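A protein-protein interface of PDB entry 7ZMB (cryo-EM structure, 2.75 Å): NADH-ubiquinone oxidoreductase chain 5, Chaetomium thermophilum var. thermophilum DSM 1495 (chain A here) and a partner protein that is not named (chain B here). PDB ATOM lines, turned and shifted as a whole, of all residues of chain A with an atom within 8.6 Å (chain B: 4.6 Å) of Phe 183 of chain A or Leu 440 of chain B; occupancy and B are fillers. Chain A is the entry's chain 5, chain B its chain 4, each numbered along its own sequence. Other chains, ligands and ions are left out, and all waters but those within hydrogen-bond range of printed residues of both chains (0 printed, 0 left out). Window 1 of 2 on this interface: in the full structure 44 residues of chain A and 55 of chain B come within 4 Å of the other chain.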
ATOM      1  N   PHE A  70      20.448 -36.886  30.665  1.00  0.00           N
ATOM      2  CA  PHE A  70      21.838 -37.135  30.297  1.00  0.00           C
ATOM      3  C   PHE A  70      22.296 -38.346  31.084  1.00  0.00           C
ATOM      4  O   PHE A  70      22.586 -38.242  32.278  1.00  0.00           O
ATOM      5  CB  PHE A  70      22.721 -35.930  30.589  1.00  0.00           C
ATOM      6  CG  PHE A  70      22.521 -34.780  29.647  1.00  0.00           C
ATOM      7  CD1 PHE A  70      21.571 -34.829  28.651  1.00  0.00           C
ATOM      8  CD2 PHE A  70      23.297 -33.641  29.765  1.00  0.00           C
ATOM      9  CE1 PHE A  70      21.391 -33.770  27.794  1.00  0.00           C
ATOM     10  CE2 PHE A  70      23.120 -32.576  28.909  1.00  0.00           C
ATOM     11  CZ  PHE A  70      22.169 -32.644  27.923  1.00  0.00           C
ATOM     12  N   TYR A 133      29.680 -40.584  22.470  1.00  0.00           N
ATOM     13  CA  TYR A 133      30.712 -39.608  22.141  1.00  0.00           C
ATOM     14  C   TYR A 133      31.545 -39.222  23.358  1.00  0.00           C
ATOM     15  O   TYR A 133      32.748 -38.972  23.233  1.00  0.00           O
ATOM     16  CB  TYR A 133      30.062 -38.375  21.522  1.00  0.00           C
ATOM     17  CG  TYR A 133      29.725 -38.577  20.076  1.00  0.00           C
ATOM     18  CD1 TYR A 133      30.716 -38.597  19.123  1.00  0.00           C
ATOM     19  CD2 TYR A 133      28.419 -38.791  19.669  1.00  0.00           C
ATOM     20  CE1 TYR A 133      30.426 -38.798  17.808  1.00  0.00           C
ATOM     21  CE2 TYR A 133      28.119 -38.993  18.348  1.00  0.00           C
ATOM     22  CZ  TYR A 133      29.135 -38.998  17.422  1.00  0.00           C
ATOM     23  OH  TYR A 133      28.861 -39.197  16.097  1.00  0.00           O
ATOM     24  N   LEU A 134      30.921 -39.143  24.538  1.00  0.00           N
ATOM     25  CA  LEU A 134      31.633 -38.676  25.722  1.00  0.00           C
ATOM     26  C   LEU A 134      32.669 -39.686  26.191  1.00  0.00           C
ATOM     27  O   LEU A 134      33.786 -39.309  26.552  1.00  0.00           O
ATOM     28  CB  LEU A 134      30.648 -38.360  26.847  1.00  0.00           C
ATOM     29  CG  LEU A 134      31.211 -37.407  27.902  1.00  0.00           C
ATOM     30  CD1 LEU A 134      31.451 -36.063  27.291  1.00  0.00           C
ATOM     31  CD2 LEU A 134      30.301 -37.287  29.086  1.00  0.00           C
ATOM     32  N   ASP A 175      40.054 -30.263  20.490  1.00  0.00           N
ATOM     33  CA  ASP A 175      39.155 -30.853  21.477  1.00  0.00           C
ATOM     34  C   ASP A 175      38.159 -29.842  22.019  1.00  0.00           C
ATOM     35  O   ASP A 175      37.117 -30.230  22.555  1.00  0.00           O
ATOM     36  CB  ASP A 175      39.950 -31.453  22.629  1.00  0.00           C
ATOM     37  CG  ASP A 175      40.725 -32.655  22.207  1.00  0.00           C
ATOM     38  OD1 ASP A 175      40.259 -33.323  21.271  1.00  0.00           O
ATOM     39  OD2 ASP A 175      41.789 -32.932  22.794  1.00  0.00           O
ATOM     40  N   CYS A 176      38.475 -28.554  21.929  1.00  0.00           N
ATOM     41  CA  CYS A 176      37.475 -27.533  22.199  1.00  0.00           C
ATOM     42  C   CYS A 176      36.330 -27.629  21.204  1.00  0.00           C
ATOM     43  O   CYS A 176      35.156 -27.638  21.586  1.00  0.00           O
ATOM     44  CB  CYS A 176      38.123 -26.148  22.154  1.00  0.00           C
ATOM     45  SG  CYS A 176      36.985 -24.773  22.338  1.00  0.00           S
ATOM     46  N   PHE A 177      36.659 -27.720  19.915  1.00  0.00           N
ATOM     47  CA  PHE A 177      35.630 -27.810  18.885  1.00  0.00           C
ATOM     48  C   PHE A 177      34.887 -29.133  18.968  1.00  0.00           C
ATOM     49  O   PHE A 177      33.679 -29.190  18.723  1.00  0.00           O
ATOM     50  CB  PHE A 177      36.257 -27.630  17.506  1.00  0.00           C
ATOM     51  CG  PHE A 177      36.675 -26.226  17.216  1.00  0.00           C
ATOM     52  CD1 PHE A 177      37.754 -25.663  17.866  1.00  0.00           C
ATOM     53  CD2 PHE A 177      35.990 -25.468  16.290  1.00  0.00           C
ATOM     54  CE1 PHE A 177      38.137 -24.376  17.604  1.00  0.00           C
ATOM     55  CE2 PHE A 177      36.369 -24.178  16.024  1.00  0.00           C
ATOM     56  CZ  PHE A 177      37.446 -23.632  16.681  1.00  0.00           C
ATOM     57  N   LEU A 178      35.591 -30.209  19.310  1.00  0.00           N
ATOM     58  CA  LEU A 178      34.912 -31.474  19.545  1.00  0.00           C
ATOM     59  C   LEU A 178      33.988 -31.385  20.752  1.00  0.00           C
ATOM     60  O   LEU A 178      32.860 -31.886  20.710  1.00  0.00           O
ATOM     61  CB  LEU A 178      35.938 -32.594  19.721  1.00  0.00           C
ATOM     62  CG  LEU A 178      35.438 -33.996  20.080  1.00  0.00           C
ATOM     63  CD1 LEU A 178      34.250 -34.409  19.235  1.00  0.00           C
ATOM     64  CD2 LEU A 178      36.555 -34.992  19.909  1.00  0.00           C
ATOM     65  N   THR A 179      34.443 -30.746  21.833  1.00  0.00           N
ATOM     66  CA  THR A 179      33.611 -30.630  23.028  1.00  0.00           C
ATOM     67  C   THR A 179      32.409 -29.728  22.781  1.00  0.00           C
ATOM     68  O   THR A 179      31.302 -30.022  23.244  1.00  0.00           O
ATOM     69  CB  THR A 179      34.441 -30.118  24.205  1.00  0.00           C
ATOM     70  OG1 THR A 179      35.294 -31.166  24.676  1.00  0.00           O
ATOM     71  CG2 THR A 179      33.549 -29.669  25.348  1.00  0.00           C
ATOM     72  N   VAL A 180      32.603 -28.630  22.052  1.00  0.00           N
ATOM     73  CA  VAL A 180      31.481 -27.762  21.717  1.00  0.00           C
ATOM     74  C   VAL A 180      30.501 -28.495  20.812  1.00  0.00           C
ATOM     75  O   VAL A 180      29.283 -28.322  20.921  1.00  0.00           O
ATOM     76  CB  VAL A 180      31.989 -26.457  21.077  1.00  0.00           C
ATOM     77  CG1 VAL A 180      30.837 -25.665  20.500  1.00  0.00           C
ATOM     78  CG2 VAL A 180      32.729 -25.630  22.097  1.00  0.00           C
ATOM     79  N   GLY A 181      31.016 -29.332  19.912  1.00  0.00           N
ATOM     80  CA  GLY A 181      30.140 -30.121  19.067  1.00  0.00           C
ATOM     81  C   GLY A 181      29.311 -31.113  19.853  1.00  0.00           C
ATOM     82  O   GLY A 181      28.128 -31.311  19.566  1.00  0.00           O
ATOM     83  N   MET A 182      29.918 -31.756  20.854  1.00  0.00           N
ATOM     84  CA  MET A 182      29.155 -32.654  21.711  1.00  0.00           C
ATOM     85  C   MET A 182      28.161 -31.891  22.574  1.00  0.00           C
ATOM     86  O   MET A 182      27.127 -32.447  22.957  1.00  0.00           O
ATOM     87  CB  MET A 182      30.090 -33.487  22.584  1.00  0.00           C
ATOM     88  CG  MET A 182      30.951 -34.467  21.827  1.00  0.00           C
ATOM     89  SD  MET A 182      31.979 -35.472  22.921  1.00  0.00           S
ATOM     90  CE  MET A 182      33.225 -34.299  23.436  1.00  0.00           C
ATOM     91  N   PHE A 183      28.447 -30.624  22.896  1.00  0.00           N
ATOM     92  CA  PHE A 183      27.436 -29.783  23.534  1.00  0.00           C
ATOM     93  C   PHE A 183      26.255 -29.546  22.608  1.00  0.00           C
ATOM     94  O   PHE A 183      25.111 -29.485  23.067  1.00  0.00           O
ATOM     95  CB  PHE A 183      28.017 -28.438  23.951  1.00  0.00           C
ATOM     96  CG  PHE A 183      28.952 -28.501  25.113  1.00  0.00           C
ATOM     97  CD1 PHE A 183      28.860 -29.507  26.044  1.00  0.00           C
ATOM     98  CD2 PHE A 183      29.922 -27.538  25.275  1.00  0.00           C
ATOM     99  CE1 PHE A 183      29.719 -29.547  27.110  1.00  0.00           C
ATOM    100  CE2 PHE A 183      30.788 -27.585  26.332  1.00  0.00           C
ATOM    101  CZ  PHE A 183      30.687 -28.594  27.248  1.00  0.00           C
ATOM    102  N   ALA A 184      26.517 -29.389  21.307  1.00  0.00           N
ATOM    103  CA  ALA A 184      25.444 -29.270  20.331  1.00  0.00           C
ATOM    104  C   ALA A 184      24.676 -30.572  20.172  1.00  0.00           C
ATOM    105  O   ALA A 184      23.473 -30.548  19.907  1.00  0.00           O
ATOM    106  CB  ALA A 184      26.010 -28.819  18.988  1.00  0.00           C
ATOM    107  N   ILE A 185      25.346 -31.714  20.320  1.00  0.00           N
ATOM    108  CA  ILE A 185      24.642 -32.991  20.264  1.00  0.00           C
ATOM    109  C   ILE A 185      23.753 -33.164  21.489  1.00  0.00           C
ATOM    110  O   ILE A 185      22.606 -33.606  21.380  1.00  0.00           O
ATOM    111  CB  ILE A 185      25.647 -34.146  20.123  1.00  0.00           C
ATOM    112  CG1 ILE A 185      26.369 -34.068  18.782  1.00  0.00           C
ATOM    113  CG2 ILE A 185      24.955 -35.474  20.281  1.00  0.00           C
ATOM    114  CD1 ILE A 185      27.179 -35.286  18.482  1.00  0.00           C
ATOM    115  N   LEU A 186      24.266 -32.820  22.670  1.00  0.00           N
ATOM    116  CA  LEU A 186      23.463 -32.904  23.888  1.00  0.00           C
ATOM    117  C   LEU A 186      22.304 -31.923  23.854  1.00  0.00           C
ATOM    118  O   LEU A 186      21.225 -32.215  24.376  1.00  0.00           O
ATOM    119  CB  LEU A 186      24.332 -32.639  25.116  1.00  0.00           C
ATOM    120  CG  LEU A 186      25.113 -33.820  25.672  1.00  0.00           C
ATOM    121  CD1 LEU A 186      25.871 -33.404  26.915  1.00  0.00           C
ATOM    122  CD2 LEU A 186      24.179 -34.968  25.972  1.00  0.00           C
ATOM    123  N   TRP A 187      22.516 -30.749  23.261  1.00  0.00           N
ATOM    124  CA  TRP A 187      21.469 -29.737  23.220  1.00  0.00           C
ATOM    125  C   TRP A 187      20.335 -30.156  22.298  1.00  0.00           C
ATOM    126  O   TRP A 187      19.159 -30.040  22.657  1.00  0.00           O
ATOM    127  CB  TRP A 187      22.057 -28.397  22.779  1.00  0.00           C
ATOM    128  CG  TRP A 187      21.141 -27.229  22.957  1.00  0.00           C
ATOM    129  CD1 TRP A 187      19.883 -27.245  23.472  1.00  0.00           C
ATOM    130  CD2 TRP A 187      21.410 -25.872  22.606  1.00  0.00           C
ATOM    131  NE1 TRP A 187      19.353 -25.986  23.468  1.00  0.00           N
ATOM    132  CE2 TRP A 187      20.272 -25.122  22.941  1.00  0.00           C
ATOM    133  CE3 TRP A 187      22.506 -25.216  22.046  1.00  0.00           C
ATOM    134  CZ2 TRP A 187      20.198 -23.753  22.734  1.00  0.00           C
ATOM    135  CZ3 TRP A 187      22.427 -23.861  21.844  1.00  0.00           C
ATOM    136  CH2 TRP A 187      21.286 -23.144  22.185  1.00  0.00           C
ATOM    137  N   SER A 188      20.663 -30.652  21.111  1.00  0.00           N
ATOM    138  CA  SER A 188      19.662 -30.874  20.080  1.00  0.00           C
ATOM    139  C   SER A 188      19.043 -32.263  20.105  1.00  0.00           C
ATOM    140  O   SER A 188      18.071 -32.495  19.379  1.00  0.00           O
ATOM    141  CB  SER A 188      20.268 -30.621  18.702  1.00  0.00           C
ATOM    142  OG  SER A 188      21.079 -31.703  18.303  1.00  0.00           O
ATOM    143  N   LEU A 189      19.538 -33.174  20.955  1.00  0.00           N
ATOM    144  CA  LEU A 189      19.014 -34.573  20.960  1.00  0.00           C
ATOM    145  C   LEU A 189      18.742 -35.063  22.383  1.00  0.00           C
ATOM    146  O   LEU A 189      17.994 -36.035  22.530  1.00  0.00           O
ATOM    147  CB  LEU A 189      19.980 -35.514  20.235  1.00  0.00           C
ATOM    148  CG  LEU A 189      19.608 -35.865  18.796  1.00  0.00           C
ATOM    149  CD1 LEU A 189      18.102 -35.819  18.607  1.00  0.00           C
ATOM    150  CD2 LEU A 189      20.292 -34.933  17.810  1.00  0.00           C
ATOM    151  N   GLY A 190      19.363 -34.443  23.383  1.00  0.00           N
ATOM    152  CA  GLY A 190      19.147 -34.824  24.788  1.00  0.00           C
ATOM    153  C   GLY A 190      20.091 -35.912  25.242  1.00  0.00           C
ATOM    154  O   GLY A 190      20.044 -36.263  26.421  1.00  0.00           O
ATOM    155  N   ASN A 191      20.874 -36.467  24.326  1.00  0.00           N
ATOM    156  CA  ASN A 191      21.903 -37.470  24.708  1.00  0.00           C
ATOM    157  C   ASN A 191      22.955 -37.536  23.608  1.00  0.00           C
ATOM    158  O   ASN A 191      22.853 -36.766  22.651  1.00  0.00           O
ATOM    159  CB  ASN A 191      21.334 -38.851  25.046  1.00  0.00           C
ATOM    160  CG  ASN A 191      22.005 -39.493  26.241  1.00  0.00           C
ATOM    161  OD1 ASN A 191      22.082 -38.897  27.312  1.00  0.00           O
ATOM    162  ND2 ASN A 191      22.487 -40.711  26.070  1.00  0.00           N
ATOM    163  N   LEU A 192      23.903 -38.444  23.750  1.00  0.00           N
ATOM    164  CA  LEU A 192      24.940 -38.677  22.758  1.00  0.00           C
ATOM    165  C   LEU A 192      25.351 -40.145  22.650  1.00  0.00           C
ATOM    166  O   LEU A 192      26.430 -40.435  22.126  1.00  0.00           O
ATOM    167  CB  LEU A 192      26.105 -37.732  23.062  1.00  0.00           C
ATOM    168  CG  LEU A 192      26.817 -37.822  24.405  1.00  0.00           C
ATOM    169  CD1 LEU A 192      27.858 -38.880  24.452  1.00  0.00           C
ATOM    170  CD2 LEU A 192      27.422 -36.466  24.719  1.00  0.00           C
ATOM    171  N   ILE A 211      26.358 -27.631  12.059  1.00  0.00           N
ATOM    172  CA  ILE A 211      27.050 -27.088  13.226  1.00  0.00           C
ATOM    173  C   ILE A 211      27.699 -28.208  14.028  1.00  0.00           C
ATOM    174  O   ILE A 211      28.848 -28.089  14.466  1.00  0.00           O
ATOM    175  CB  ILE A 211      26.095 -26.224  14.076  1.00  0.00           C
ATOM    176  CG1 ILE A 211      26.887 -25.413  15.101  1.00  0.00           C
ATOM    177  CG2 ILE A 211      25.048 -27.058  14.781  1.00  0.00           C
ATOM    178  CD1 ILE A 211      27.793 -24.378  14.482  1.00  0.00           C
ATOM    179  N   ILE A 212      26.990 -29.322  14.209  1.00  0.00           N
ATOM    180  CA  ILE A 212      27.590 -30.495  14.835  1.00  0.00           C
ATOM    181  C   ILE A 212      28.683 -31.067  13.944  1.00  0.00           C
ATOM    182  O   ILE A 212      29.793 -31.358  14.403  1.00  0.00           O
ATOM    183  CB  ILE A 212      26.513 -31.549  15.134  1.00  0.00           C
ATOM    184  CG1 ILE A 212      25.676 -31.130  16.336  1.00  0.00           C
ATOM    185  CG2 ILE A 212      27.152 -32.912  15.341  1.00  0.00           C
ATOM    186  CD1 ILE A 212      24.395 -31.897  16.472  1.00  0.00           C
ATOM    187  N   CYS A 215      31.934 -28.956  13.839  1.00  0.00           N
ATOM    188  CA  CYS A 215      32.729 -29.008  15.061  1.00  0.00           C
ATOM    189  C   CYS A 215      33.576 -30.268  15.119  1.00  0.00           C
ATOM    190  O   CYS A 215      34.769 -30.216  15.440  1.00  0.00           O
ATOM    191  CB  CYS A 215      31.817 -28.914  16.274  1.00  0.00           C
ATOM    192  SG  CYS A 215      31.393 -27.231  16.734  1.00  0.00           S
ATOM    193  N   ILE B 353      33.930 -20.270  35.462  1.00  0.00           N
ATOM    194  CA  ILE B 353      33.153 -21.292  34.761  1.00  0.00           C
ATOM    195  C   ILE B 353      31.972 -21.749  35.601  1.00  0.00           C
ATOM    196  O   ILE B 353      30.859 -21.897  35.086  1.00  0.00           O
ATOM    197  CB  ILE B 353      34.019 -22.491  34.319  1.00  0.00           C
ATOM    198  CG1 ILE B 353      35.042 -22.103  33.266  1.00  0.00           C
ATOM    199  CG2 ILE B 353      33.162 -23.611  33.767  1.00  0.00           C
ATOM    200  CD1 ILE B 353      36.317 -21.700  33.789  1.00  0.00           C
ATOM    201  N   GLU B 436      33.397 -28.982  34.707  1.00  0.00           N
ATOM    202  CA  GLU B 436      33.626 -28.046  33.578  1.00  0.00           C
ATOM    203  C   GLU B 436      32.687 -28.401  32.425  1.00  0.00           C
ATOM    204  O   GLU B 436      32.048 -27.492  31.903  1.00  0.00           O
ATOM    205  CB  GLU B 436      35.075 -28.204  33.119  1.00  0.00           C
ATOM    206  CG  GLU B 436      35.520 -27.178  32.097  1.00  0.00           C
ATOM    207  CD  GLU B 436      36.178 -25.933  32.667  1.00  0.00           C
ATOM    208  OE1 GLU B 436      36.510 -25.033  31.873  1.00  0.00           O
ATOM    209  OE2 GLU B 436      36.368 -25.870  33.899  1.00  0.00           O
ATOM    210  N   PHE B 437      32.555 -29.690  32.098  1.00  0.00           N
ATOM    211  CA  PHE B 437      31.742 -30.110  30.928  1.00  0.00           C
ATOM    212  C   PHE B 437      30.278 -29.770  31.174  1.00  0.00           C
ATOM    213  O   PHE B 437      29.624 -29.241  30.273  1.00  0.00           O
ATOM    214  CB  PHE B 437      31.916 -31.607  30.666  1.00  0.00           C
ATOM    215  CG  PHE B 437      31.248 -32.100  29.409  1.00  0.00           C
ATOM    216  CD1 PHE B 437      31.906 -32.051  28.191  1.00  0.00           C
ATOM    217  CD2 PHE B 437      29.959 -32.607  29.441  1.00  0.00           C
ATOM    218  CE1 PHE B 437      31.289 -32.493  27.033  1.00  0.00           C
ATOM    219  CE2 PHE B 437      29.342 -33.047  28.282  1.00  0.00           C
ATOM    220  CZ  PHE B 437      30.007 -32.986  27.079  1.00  0.00           C
ATOM    221  N   MET B 438      29.785 -30.085  32.365  1.00  0.00           N
ATOM    222  CA  MET B 438      28.383 -29.843  32.673  1.00  0.00           C
ATOM    223  C   MET B 438      28.091 -28.357  32.836  1.00  0.00           C
ATOM    224  O   MET B 438      27.005 -27.894  32.477  1.00  0.00           O
ATOM    225  CB  MET B 438      27.998 -30.618  33.921  1.00  0.00           C
ATOM    226  CG  MET B 438      28.017 -32.105  33.746  1.00  0.00           C
ATOM    227  SD  MET B 438      27.633 -32.864  35.323  1.00  0.00           S
ATOM    228  CE  MET B 438      25.918 -32.439  35.471  1.00  0.00           C
ATOM    229  N   SER B 439      29.039 -27.591  33.379  1.00  0.00           N
ATOM    230  CA  SER B 439      28.847 -26.145  33.458  1.00  0.00           C
ATOM    231  C   SER B 439      28.870 -25.511  32.076  1.00  0.00           C
ATOM    232  O   SER B 439      28.093 -24.596  31.796  1.00  0.00           O
ATOM    233  CB  SER B 439      29.914 -25.503  34.344  1.00  0.00           C
ATOM    234  OG  SER B 439      29.862 -25.989  35.663  1.00  0.00           O
ATOM    235  N   LEU B 440      29.760 -25.984  31.204  1.00  0.00           N
ATOM    236  CA  LEU B 440      29.909 -25.377  29.889  1.00  0.00           C
ATOM    237  C   LEU B 440      28.714 -25.680  28.999  1.00  0.00           C
ATOM    238  O   LEU B 440      28.288 -24.827  28.216  1.00  0.00           O
ATOM    239  CB  LEU B 440      31.202 -25.851  29.239  1.00  0.00           C
ATOM    240  CG  LEU B 440      32.510 -25.228  29.718  1.00  0.00           C
ATOM    241  CD1 LEU B 440      33.663 -25.999  29.155  1.00  0.00           C
ATOM    242  CD2 LEU B 440      32.612 -23.774  29.333  1.00  0.00           C
ATOM    243  N   TYR B 441      28.158 -26.886  29.098  1.00  0.00           N
ATOM    244  CA  TYR B 441      26.929 -27.158  28.367  1.00  0.00           C
ATOM    245  C   TYR B 441      25.808 -26.246  28.839  1.00  0.00           C
ATOM    246  O   TYR B 441      25.063 -25.695  28.023  1.00  0.00           O
ATOM    247  CB  TYR B 441      26.514 -28.618  28.525  1.00  0.00           C
ATOM    248  CG  TYR B 441      25.102 -28.861  28.050  1.00  0.00           C
ATOM    249  CD1 TYR B 441      24.837 -29.080  26.714  1.00  0.00           C
ATOM    250  CD2 TYR B 441      24.031 -28.834  28.933  1.00  0.00           C
ATOM    251  CE1 TYR B 441      23.559 -29.280  26.273  1.00  0.00           C
ATOM    252  CE2 TYR B 441      22.750 -29.029  28.496  1.00  0.00           C
ATOM    253  CZ  TYR B 441      22.520 -29.251  27.166  1.00  0.00           C
ATOM    254  OH  TYR B 441      21.243 -29.457  26.715  1.00  0.00           O
ATOM    255  N   GLY B 442      25.664 -26.087  30.154  1.00  0.00           N
ATOM    256  CA  GLY B 442      24.645 -25.194  30.669  1.00  0.00           C
ATOM    257  C   GLY B 442      24.875 -23.756  30.257  1.00  0.00           C
ATOM    258  O   GLY B 442      23.935 -23.048  29.891  1.00  0.00           O
ATOM    259  N   THR B 443      26.126 -23.304  30.310  1.00  0.00           N
ATOM    260  CA  THR B 443      26.435 -21.944  29.889  1.00  0.00           C
ATOM    261  C   THR B 443      26.131 -21.754  28.413  1.00  0.00           C
ATOM    262  O   THR B 443      25.516 -20.762  28.017  1.00  0.00           O
ATOM    263  CB  THR B 443      27.901 -21.620  30.191  1.00  0.00           C
ATOM    264  OG1 THR B 443      28.180 -21.912  31.563  1.00  0.00           O
ATOM    265  CG2 THR B 443      28.189 -20.156  29.933  1.00  0.00           C
ATOM    266  N   LEU B 444      26.546 -22.713  27.587  1.00  0.00           N
ATOM    267  CA  LEU B 444      26.304 -22.634  26.150  1.00  0.00           C
ATOM    268  C   LEU B 444      24.818 -22.700  25.839  1.00  0.00           C
ATOM    269  O   LEU B 444      24.304 -21.910  25.040  1.00  0.00           O
ATOM    270  CB  LEU B 444      27.048 -23.768  25.448  1.00  0.00           C
ATOM    271  CG  LEU B 444      26.990 -23.844  23.929  1.00  0.00           C
ATOM    272  CD1 LEU B 444      27.626 -22.623  23.323  1.00  0.00           C
ATOM    273  CD2 LEU B 444      27.678 -25.075  23.443  1.00  0.00           C
ATOM    274  N   GLY B 451      28.944 -19.137  26.328  1.00  0.00           N
ATOM    275  CA  GLY B 451      29.477 -20.466  26.555  1.00  0.00           C
ATOM    276  C   GLY B 451      30.617 -20.793  25.615  1.00  0.00           C
ATOM    277  O   GLY B 451      31.580 -21.459  26.000  1.00  0.00           O
ATOM    278  N   ALA B 454      33.427 -19.004  26.886  1.00  0.00           N
ATOM    279  CA  ALA B 454      33.873 -19.772  28.043  1.00  0.00           C
ATOM    280  C   ALA B 454      34.586 -21.046  27.609  1.00  0.00           C
ATOM    281  O   ALA B 454      35.548 -21.475  28.252  1.00  0.00           O
ATOM    282  CB  ALA B 454      32.684 -20.096  28.945  1.00  0.00           C
ATOM    283  N   SER B 455      34.151 -21.644  26.500  1.00  0.00           N
ATOM    284  CA  SER B 455      34.689 -22.903  26.004  1.00  0.00           C
ATOM    285  C   SER B 455      36.139 -22.798  25.575  1.00  0.00           C
ATOM    286  O   SER B 455      36.780 -23.829  25.351  1.00  0.00           O
ATOM    287  CB  SER B 455      33.845 -23.407  24.840  1.00  0.00           C
ATOM    288  OG  SER B 455      34.167 -22.721  23.645  1.00  0.00           O
ATOM    289  N   ILE B 458      39.064 -24.822  27.691  1.00  0.00           N
ATOM    290  CA  ILE B 458      39.701 -26.090  27.352  1.00  0.00           C
ATOM    291  C   ILE B 458      41.052 -25.840  26.703  1.00  0.00           C
ATOM    292  O   ILE B 458      42.040 -26.518  27.007  1.00  0.00           O
ATOM    293  CB  ILE B 458      38.784 -26.939  26.448  1.00  0.00           C
ATOM    294  CG1 ILE B 458      37.490 -27.310  27.172  1.00  0.00           C
ATOM    295  CG2 ILE B 458      39.494 -28.185  25.963  1.00  0.00           C
ATOM    296  CD1 ILE B 458      36.386 -26.318  27.020  1.00  0.00           C
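O of Ser 455 of chain B sits at hydrogen-bond distance from SG of Cys 176 of chain A, 3.2 Å away.
The backbone carbonyl oxygen (O) of Asp 175 of chain A lies within hydrogen-bond range of the side-chain hydroxyl (OG1) of Thr 179 of chain A.
Among the printed residues, pairs that only touch across the chains: Phe 183 of chain A with Phe 437 of chain B (3.2 Å), Leu 134 of chain A with Phe 437 of chain B (3.4 Å), Phe 183 of chain A with Leu 440 of chain B (3.4 Å), Phe 183 of chain A with Leu 444 of chain B (3.4 Å), Phe 70 of chain A with Tyr 441 of chain B (3.5 Å), Trp 187 of chain A with Tyr 441 of chain B (3.5 Å), Phe 183 of chain A with Tyr 441 of chain B (3.5 Å), Val 180 of chain A with Ser 455 of chain B (3.6 Å), Leu 186 of chain A with Tyr 441 of chain B (3.6 Å), Leu 186 of chain A with Phe 437 of chain B (3.7 Å) and Thr 179 of chain A with Phe 437 of chain B (3.99 Å).
Printed residues of chain B within 4 Å of Val 180 of chain A: Ser 455 (3.6 Å).
Of chain B, only Phe 437, Leu 440, Tyr 441 and Leu 444 come within 4 Å of Phe 183 of chain A.
Of the printed residues of chain B, Trp 187 of chain A touches Tyr 441.
Leu 189 of chain A touches none of the printed residues of chain B.
Printed residues of chain A within 4 Å of Phe 437 of chain B: Leu 134 (3.4 Å), Thr 179 (3.99 Å), Phe 183 (3.2 Å) and Leu 186 (3.7 Å).
Of chain A, only Phe 183 (3.4 Å) comes within 4 Å of Leu 440 of chain B.
Printed residues of chain A within 4 Å of Tyr 441 of chain B: Phe 70 (3.5 Å), Phe 183 (3.5 Å), Leu 186 (3.6 Å) and Trp 187 (3.5 Å).
The nearest printed residue of chain B that does not touch Leu 134 of chain A is Met 438 of chain B (7.3 Å).
Printed residues of chain A that touch a printed residue of chain B: Phe 70, Leu 134, Cys 176, Thr 179, Val 180, Phe 183, Leu 186 and Trp 187.
Hydrophobic or aromatic side chains of chain A that line the printed part of chain B: Phe 70, Leu 134, Val 180, Phe 183, Leu 186 and Trp 187.
Of the 14 printed residues of chain B, 5 touch a printed residue of chain A.
Printed residues of chain B that touch a printed residue of chain A: Phe 437, Leu 440, Tyr 441, Leu 444 and Ser 455.
Hydrophobic or aromatic side chains of chain B that line the printed part of chain A: Phe 437, Leu 440, Tyr 441 and Leu 444.
Among the printed residues, 12 pairs touch across the chains.
Among the printed residues, no Asp or Glu carboxylate lies within 4 Å of a Lys or Arg side-chain nitrogen of the other chain.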
